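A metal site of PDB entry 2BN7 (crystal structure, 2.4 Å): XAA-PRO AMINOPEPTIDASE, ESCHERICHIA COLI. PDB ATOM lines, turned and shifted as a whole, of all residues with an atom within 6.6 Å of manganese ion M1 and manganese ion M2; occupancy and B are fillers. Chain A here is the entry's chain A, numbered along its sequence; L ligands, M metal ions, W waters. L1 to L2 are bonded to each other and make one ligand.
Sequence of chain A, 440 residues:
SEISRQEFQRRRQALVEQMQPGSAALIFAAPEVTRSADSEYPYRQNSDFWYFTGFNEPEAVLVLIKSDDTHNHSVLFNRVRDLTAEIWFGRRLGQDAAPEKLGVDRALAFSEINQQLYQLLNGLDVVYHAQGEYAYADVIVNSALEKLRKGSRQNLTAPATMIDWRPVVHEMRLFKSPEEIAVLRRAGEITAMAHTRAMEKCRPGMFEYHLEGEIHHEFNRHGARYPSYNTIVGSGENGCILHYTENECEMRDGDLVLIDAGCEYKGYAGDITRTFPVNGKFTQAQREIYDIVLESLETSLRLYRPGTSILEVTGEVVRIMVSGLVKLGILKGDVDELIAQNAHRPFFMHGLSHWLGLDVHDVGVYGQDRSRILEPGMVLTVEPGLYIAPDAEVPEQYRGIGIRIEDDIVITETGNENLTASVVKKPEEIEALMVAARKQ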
ATOM      1  N   TYR A 229       4.729   2.476  26.113  1.00  0.00           N
ATOM      2  CA  TYR A 229       4.920   3.621  25.235  1.00  0.00           C
ATOM      3  C   TYR A 229       4.178   3.385  23.927  1.00  0.00           C
ATOM      4  O   TYR A 229       3.774   2.259  23.628  1.00  0.00           O
ATOM      5  CB  TYR A 229       6.416   3.873  24.958  1.00  0.00           C
ATOM      6  CG  TYR A 229       7.172   2.657  24.473  1.00  0.00           C
ATOM      7  CD1 TYR A 229       7.605   1.696  25.379  1.00  0.00           C
ATOM      8  CD2 TYR A 229       7.445   2.465  23.128  1.00  0.00           C
ATOM      9  CE1 TYR A 229       8.287   0.578  24.955  1.00  0.00           C
ATOM     10  CE2 TYR A 229       8.124   1.354  22.689  1.00  0.00           C
ATOM     11  CZ  TYR A 229       8.558   0.407  23.615  1.00  0.00           C
ATOM     12  OH  TYR A 229       9.239  -0.697  23.211  1.00  0.00           O
ATOM     13  N   ILE A 232       5.822   1.618  17.798  1.00  0.00           N
ATOM     14  CA  ILE A 232       6.503   2.085  16.608  1.00  0.00           C
ATOM     15  C   ILE A 232       6.601   0.929  15.616  1.00  0.00           C
ATOM     16  O   ILE A 232       7.187  -0.098  15.923  1.00  0.00           O
ATOM     17  CB  ILE A 232       7.949   2.577  16.950  1.00  0.00           C
ATOM     18  CG1 ILE A 232       7.896   3.854  17.805  1.00  0.00           C
ATOM     19  CG2 ILE A 232       8.802   2.790  15.691  1.00  0.00           C
ATOM     20  CD1 ILE A 232       9.033   3.958  18.798  1.00  0.00           C
ATOM     21  N   ASP A 260       9.422  -1.230  17.429  1.00  0.00           N
ATOM     22  CA  ASP A 260       9.773  -0.920  18.808  1.00  0.00           C
ATOM     23  C   ASP A 260       8.481  -0.880  19.636  1.00  0.00           C
ATOM     24  O   ASP A 260       7.654   0.025  19.479  1.00  0.00           O
ATOM     25  CB  ASP A 260      10.524   0.411  18.887  1.00  0.00           C
ATOM     26  CG  ASP A 260      11.302   0.572  20.179  1.00  0.00           C
ATOM     27  OD1 ASP A 260      11.037  -0.132  21.174  1.00  0.00           O
ATOM     28  OD2 ASP A 260      12.200   1.438  20.194  1.00  0.00           O
ATOM     29  N   ALA A 261       8.311  -1.885  20.494  1.00  0.00           N
ATOM     30  CA  ALA A 261       7.075  -2.004  21.279  1.00  0.00           C
ATOM     31  C   ALA A 261       7.318  -2.733  22.605  1.00  0.00           C
ATOM     32  O   ALA A 261       8.138  -3.629  22.695  1.00  0.00           O
ATOM     33  CB  ALA A 261       5.993  -2.725  20.450  1.00  0.00           C
ATOM     34  N   ASP A 271      10.510  -3.352  26.701  1.00  0.00           N
ATOM     35  CA  ASP A 271      10.987  -2.457  25.651  1.00  0.00           C
ATOM     36  C   ASP A 271      11.865  -3.226  24.669  1.00  0.00           C
ATOM     37  O   ASP A 271      13.079  -3.364  24.873  1.00  0.00           O
ATOM     38  CB  ASP A 271      11.759  -1.289  26.272  1.00  0.00           C
ATOM     39  CG  ASP A 271      12.171  -0.263  25.259  1.00  0.00           C
ATOM     40  OD1 ASP A 271      11.843  -0.444  24.069  1.00  0.00           O
ATOM     41  OD2 ASP A 271      12.838   0.710  25.652  1.00  0.00           O
ATOM     42  N   ILE A 272      11.240  -3.725  23.609  1.00  0.00           N
ATOM     43  CA  ILE A 272      11.945  -4.521  22.610  1.00  0.00           C
ATOM     44  C   ILE A 272      11.864  -3.848  21.230  1.00  0.00           C
ATOM     45  O   ILE A 272      10.830  -3.274  20.857  1.00  0.00           O
ATOM     46  CB  ILE A 272      11.350  -5.949  22.515  1.00  0.00           C
ATOM     47  CG1 ILE A 272      11.619  -6.727  23.805  1.00  0.00           C
ATOM     48  CG2 ILE A 272      11.936  -6.700  21.299  1.00  0.00           C
ATOM     49  CD1 ILE A 272      11.107  -8.172  23.778  1.00  0.00           C
ATOM     50  N   THR A 273      12.972  -3.926  20.493  1.00  0.00           N
ATOM     51  CA  THR A 273      12.968  -3.590  19.078  1.00  0.00           C
ATOM     52  C   THR A 273      13.477  -4.797  18.315  1.00  0.00           C
ATOM     53  O   THR A 273      14.481  -5.408  18.689  1.00  0.00           O
ATOM     54  CB  THR A 273      13.827  -2.347  18.699  1.00  0.00           C
ATOM     55  OG1 THR A 273      13.506  -1.250  19.551  1.00  0.00           O
ATOM     56  CG2 THR A 273      13.527  -1.930  17.264  1.00  0.00           C
ATOM     57  N   HIS A 354      19.243   2.926  27.973  1.00  0.00           N
ATOM     58  CA  HIS A 354      18.618   3.751  28.992  1.00  0.00           C
ATOM     59  C   HIS A 354      18.138   2.869  30.133  1.00  0.00           C
ATOM     60  O   HIS A 354      17.936   1.666  29.950  1.00  0.00           O
ATOM     61  CB  HIS A 354      17.462   4.607  28.433  1.00  0.00           C
ATOM     62  CG  HIS A 354      16.385   3.823  27.754  1.00  0.00           C
ATOM     63  ND1 HIS A 354      15.419   3.112  28.444  1.00  0.00           N
ATOM     64  CD2 HIS A 354      16.089   3.671  26.443  1.00  0.00           C
ATOM     65  CE1 HIS A 354      14.597   2.541  27.585  1.00  0.00           C
ATOM     66  NE2 HIS A 354      14.980   2.863  26.356  1.00  0.00           N
ATOM     67  N   LEU A 356      15.564   1.193  32.729  1.00  0.00           N
ATOM     68  CA  LEU A 356      14.231   0.633  32.470  1.00  0.00           C
ATOM     69  C   LEU A 356      13.538   0.258  33.785  1.00  0.00           C
ATOM     70  O   LEU A 356      14.154  -0.341  34.680  1.00  0.00           O
ATOM     71  CB  LEU A 356      14.359  -0.614  31.584  1.00  0.00           C
ATOM     72  CG  LEU A 356      13.052  -1.253  31.101  1.00  0.00           C
ATOM     73  CD1 LEU A 356      12.319  -0.344  30.111  1.00  0.00           C
ATOM     74  CD2 LEU A 356      13.348  -2.606  30.466  1.00  0.00           C
ATOM     75  N   VAL A 360       9.548   3.612  30.898  1.00  0.00           N
ATOM     76  CA  VAL A 360      10.344   2.974  29.857  1.00  0.00           C
ATOM     77  C   VAL A 360      11.720   3.650  29.794  1.00  0.00           C
ATOM     78  O   VAL A 360      12.744   2.974  29.833  1.00  0.00           O
ATOM     79  CB  VAL A 360       9.574   2.904  28.485  1.00  0.00           C
ATOM     80  CG1 VAL A 360       9.246   4.292  27.933  1.00  0.00           C
ATOM     81  CG2 VAL A 360      10.370   2.082  27.471  1.00  0.00           C
ATOM     82  N   HIS A 361      11.750   4.981  29.744  1.00  0.00           N
ATOM     83  CA  HIS A 361      12.977   5.735  29.985  1.00  0.00           C
ATOM     84  C   HIS A 361      13.007   6.079  31.469  1.00  0.00           C
ATOM     85  O   HIS A 361      12.463   7.105  31.889  1.00  0.00           O
ATOM     86  CB  HIS A 361      13.014   7.015  29.155  1.00  0.00           C
ATOM     87  CG  HIS A 361      12.969   6.767  27.689  1.00  0.00           C
ATOM     88  ND1 HIS A 361      12.565   7.731  26.786  1.00  0.00           N
ATOM     89  CD2 HIS A 361      13.238   5.665  26.960  1.00  0.00           C
ATOM     90  CE1 HIS A 361      12.617   7.232  25.564  1.00  0.00           C
ATOM     91  NE2 HIS A 361      13.027   5.976  25.646  1.00  0.00           N
ATOM     92  N   THR A 381      18.287  -0.977  28.805  1.00  0.00           N
ATOM     93  CA  THR A 381      18.120  -1.464  27.457  1.00  0.00           C
ATOM     94  C   THR A 381      19.478  -1.529  26.768  1.00  0.00           C
ATOM     95  O   THR A 381      20.448  -0.939  27.235  1.00  0.00           O
ATOM     96  CB  THR A 381      17.192  -0.562  26.647  1.00  0.00           C
ATOM     97  OG1 THR A 381      17.804   0.717  26.452  1.00  0.00           O
ATOM     98  CG2 THR A 381      15.853  -0.426  27.380  1.00  0.00           C
ATOM     99  N   VAL A 382      19.524  -2.299  25.688  1.00  0.00           N
ATOM    100  CA  VAL A 382      20.702  -2.395  24.840  1.00  0.00           C
ATOM    101  C   VAL A 382      20.160  -2.331  23.429  1.00  0.00           C
ATOM    102  O   VAL A 382      19.586  -3.307  22.953  1.00  0.00           O
ATOM    103  CB  VAL A 382      21.508  -3.710  25.072  1.00  0.00           C
ATOM    104  CG1 VAL A 382      22.860  -3.660  24.356  1.00  0.00           C
ATOM    105  CG2 VAL A 382      21.726  -3.958  26.552  1.00  0.00           C
ATOM    106  N   GLU A 383      20.327  -1.196  22.779  1.00  0.00           N
ATOM    107  CA  GLU A 383      19.649  -0.929  21.504  1.00  0.00           C
ATOM    108  C   GLU A 383      20.493  -0.183  20.482  1.00  0.00           C
ATOM    109  O   GLU A 383      20.191   0.959  20.129  1.00  0.00           O
ATOM    110  CB  GLU A 383      18.347  -0.168  21.769  1.00  0.00           C
ATOM    111  CG  GLU A 383      18.483   1.074  22.620  1.00  0.00           C
ATOM    112  CD  GLU A 383      17.156   1.722  22.879  1.00  0.00           C
ATOM    113  OE1 GLU A 383      16.405   1.943  21.888  1.00  0.00           O
ATOM    114  OE2 GLU A 383      16.866   2.003  24.056  1.00  0.00           O
ATOM    115  N   ARG A 404      17.118  -1.219  14.085  1.00  0.00           N
ATOM    116  CA  ARG A 404      17.448  -1.234  15.510  1.00  0.00           C
ATOM    117  C   ARG A 404      17.140  -2.633  16.037  1.00  0.00           C
ATOM    118  O   ARG A 404      16.184  -3.270  15.584  1.00  0.00           O
ATOM    119  CB  ARG A 404      16.658  -0.179  16.279  1.00  0.00           C
ATOM    120  CG  ARG A 404      16.893  -0.170  17.791  1.00  0.00           C
ATOM    121  CD  ARG A 404      16.470   1.149  18.445  1.00  0.00           C
ATOM    122  NE  ARG A 404      15.023   1.434  18.371  1.00  0.00           N
ATOM    123  CZ  ARG A 404      14.440   2.275  17.505  1.00  0.00           C
ATOM    124  NH1 ARG A 404      15.134   2.959  16.601  1.00  0.00           N
ATOM    125  NH2 ARG A 404      13.134   2.444  17.559  1.00  0.00           N
ATOM    126  N   GLU A 406      16.904  -4.244  19.926  1.00  0.00           N
ATOM    127  CA  GLU A 406      16.900  -3.851  21.329  1.00  0.00           C
ATOM    128  C   GLU A 406      16.464  -4.966  22.270  1.00  0.00           C
ATOM    129  O   GLU A 406      15.364  -5.522  22.130  1.00  0.00           O
ATOM    130  CB  GLU A 406      15.973  -2.649  21.518  1.00  0.00           C
ATOM    131  CG  GLU A 406      15.666  -2.299  22.971  1.00  0.00           C
ATOM    132  CD  GLU A 406      14.890  -1.027  23.090  1.00  0.00           C
ATOM    133  OE1 GLU A 406      14.125  -0.716  22.144  1.00  0.00           O
ATOM    134  OE2 GLU A 406      15.036  -0.342  24.121  1.00  0.00           O
ATOM    135  N   ASP A 408      16.379  -6.056  26.701  1.00  0.00           N
ATOM    136  CA  ASP A 408      16.314  -5.529  28.069  1.00  0.00           C
ATOM    137  C   ASP A 408      17.108  -6.443  28.988  1.00  0.00           C
ATOM    138  O   ASP A 408      16.931  -7.653  28.966  1.00  0.00           O
ATOM    139  CB  ASP A 408      14.861  -5.504  28.566  1.00  0.00           C
ATOM    140  CG  ASP A 408      13.954  -4.719  27.663  1.00  0.00           C
ATOM    141  OD1 ASP A 408      14.450  -3.807  26.957  1.00  0.00           O
ATOM    142  OD2 ASP A 408      12.743  -5.025  27.670  1.00  0.00           O
HETATM  143  N1  LIG L   1      14.281   4.757  21.706  1.00  0.00           N
HETATM  144  C1  LIG L   1      15.611   5.192  22.099  1.00  0.00           C
HETATM  145  C2  LIG L   1      15.637   6.445  22.987  1.00  0.00           C
HETATM  146  O1  LIG L   1      14.642   7.176  23.073  1.00  0.00           O
HETATM  147  C3  LIG L   1      16.289   5.501  20.760  1.00  0.00           C
HETATM  148  C4  LIG L   1      15.544   4.720  19.759  1.00  0.00           C
HETATM  149  C5  LIG L   1      14.145   4.667  20.241  1.00  0.00           C
HETATM  150  N1  LG2 L   2      16.780   6.664  23.632  1.00  0.00           N
HETATM  151  C1  LG2 L   2      17.067   7.877  24.410  1.00  0.00           C
HETATM  152  C2  LG2 L   2      18.426   8.420  23.979  1.00  0.00           C
HETATM  153  O1  LG2 L   2      18.653   9.623  23.872  1.00  0.00           O
HETATM  154  C3  LG2 L   2      17.065   7.575  25.921  1.00  0.00           C
HETATM  155  C4  LG2 L   2      17.259   8.762  26.891  1.00  0.00           C
HETATM  156  C5  LG2 L   2      16.079   9.714  26.871  1.00  0.00           C
HETATM  157  C6  LG2 L   2      17.490   8.264  28.298  1.00  0.00           C
HETATM  158  O2  LG2 L   2      19.352   7.642  23.725  1.00  0.00           O
HETATM  159 MN    MN M   1      12.558   0.696  22.455  1.00  0.00          MN
HETATM  160 MN    MN M   2      14.610   1.612  24.644  1.00  0.00          MN
HETATM  161 ZN    ZN M   3      12.580   5.824  23.204  1.00  0.00          ZN
HETATM  162  O   HOH W   1      10.934   3.395  23.470  1.00  0.00           O
HETATM  163  O   HOH W   2      13.917   2.349  22.925  1.00  0.00           O
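OE1 of Glu 383 sits close to N1 of LIG L1 (3.5 Å).
The backbone NH (N) of Thr 381 lies within hydrogen-bond range of the backbone carbonyl oxygen (O) of His 354.
The backbone carbonyl oxygen (O) of Ile 232 lies within hydrogen-bond range of the backbone NH (N) of Asp 260 (2.9 Å).
The side-chain hydroxyl of Thr 273 is in hydrogen-bond range of the guanidinium group of Arg 404 (3.3 Å).
The side-chain carboxylate (OD1) of Asp 271 lies close to the side-chain hydroxyl (OH) of Tyr 229.
The side-chain hydroxyl (OG1) of Thr 381 lies close to the side-chain carboxylate (OE2) of Glu 383, at 2.9 Å.
OD2 of Asp 260 sits close to OG1 of Thr 273.
A ring nitrogen (ND1) of His 354 lies close to the backbone carbonyl oxygen of Val 360, 3.0 Å away.
The guanidinium group (NH2) of Arg 404 lies close to the side-chain carboxylate (OD2) of Asp 260 (3.0 Å).
Merely in contact with manganese ion M1: Tyr 229 (3.7 Å) and Thr 273 (3.6 Å).
Within 4 Å of manganese ion M1: Tyr 229, Asp 260, Asp 271, Thr 273 and Glu 406.
Residues that only touch manganese ion M2: Thr 381 (3.6 Å).
Manganese ion M1 is bound by the side-chain carboxylate (OD1) of Asp 271 (2.1 Å), the side-chain carboxylate (OE1) of Glu 406 (2.1 Å), the side-chain carboxylate (OD1) of Asp 260 (2.2 Å), water W2 (2.2 Å) and the side-chain carboxylate (OD2) of Asp 260 (2.4 Å).
Manganese ion M1 has five donor atoms within binding distance.
Manganese ion M2 is bound by water W2 (2.0 Å), OE2 of Glu 406 (2.1 Å), NE2 of His 354 (2.2 Å), OD2 of Asp 271 (2.2 Å) and OE2 of Glu 383 (2.4 Å).
Manganese ion M2 has five donor atoms within binding distance.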
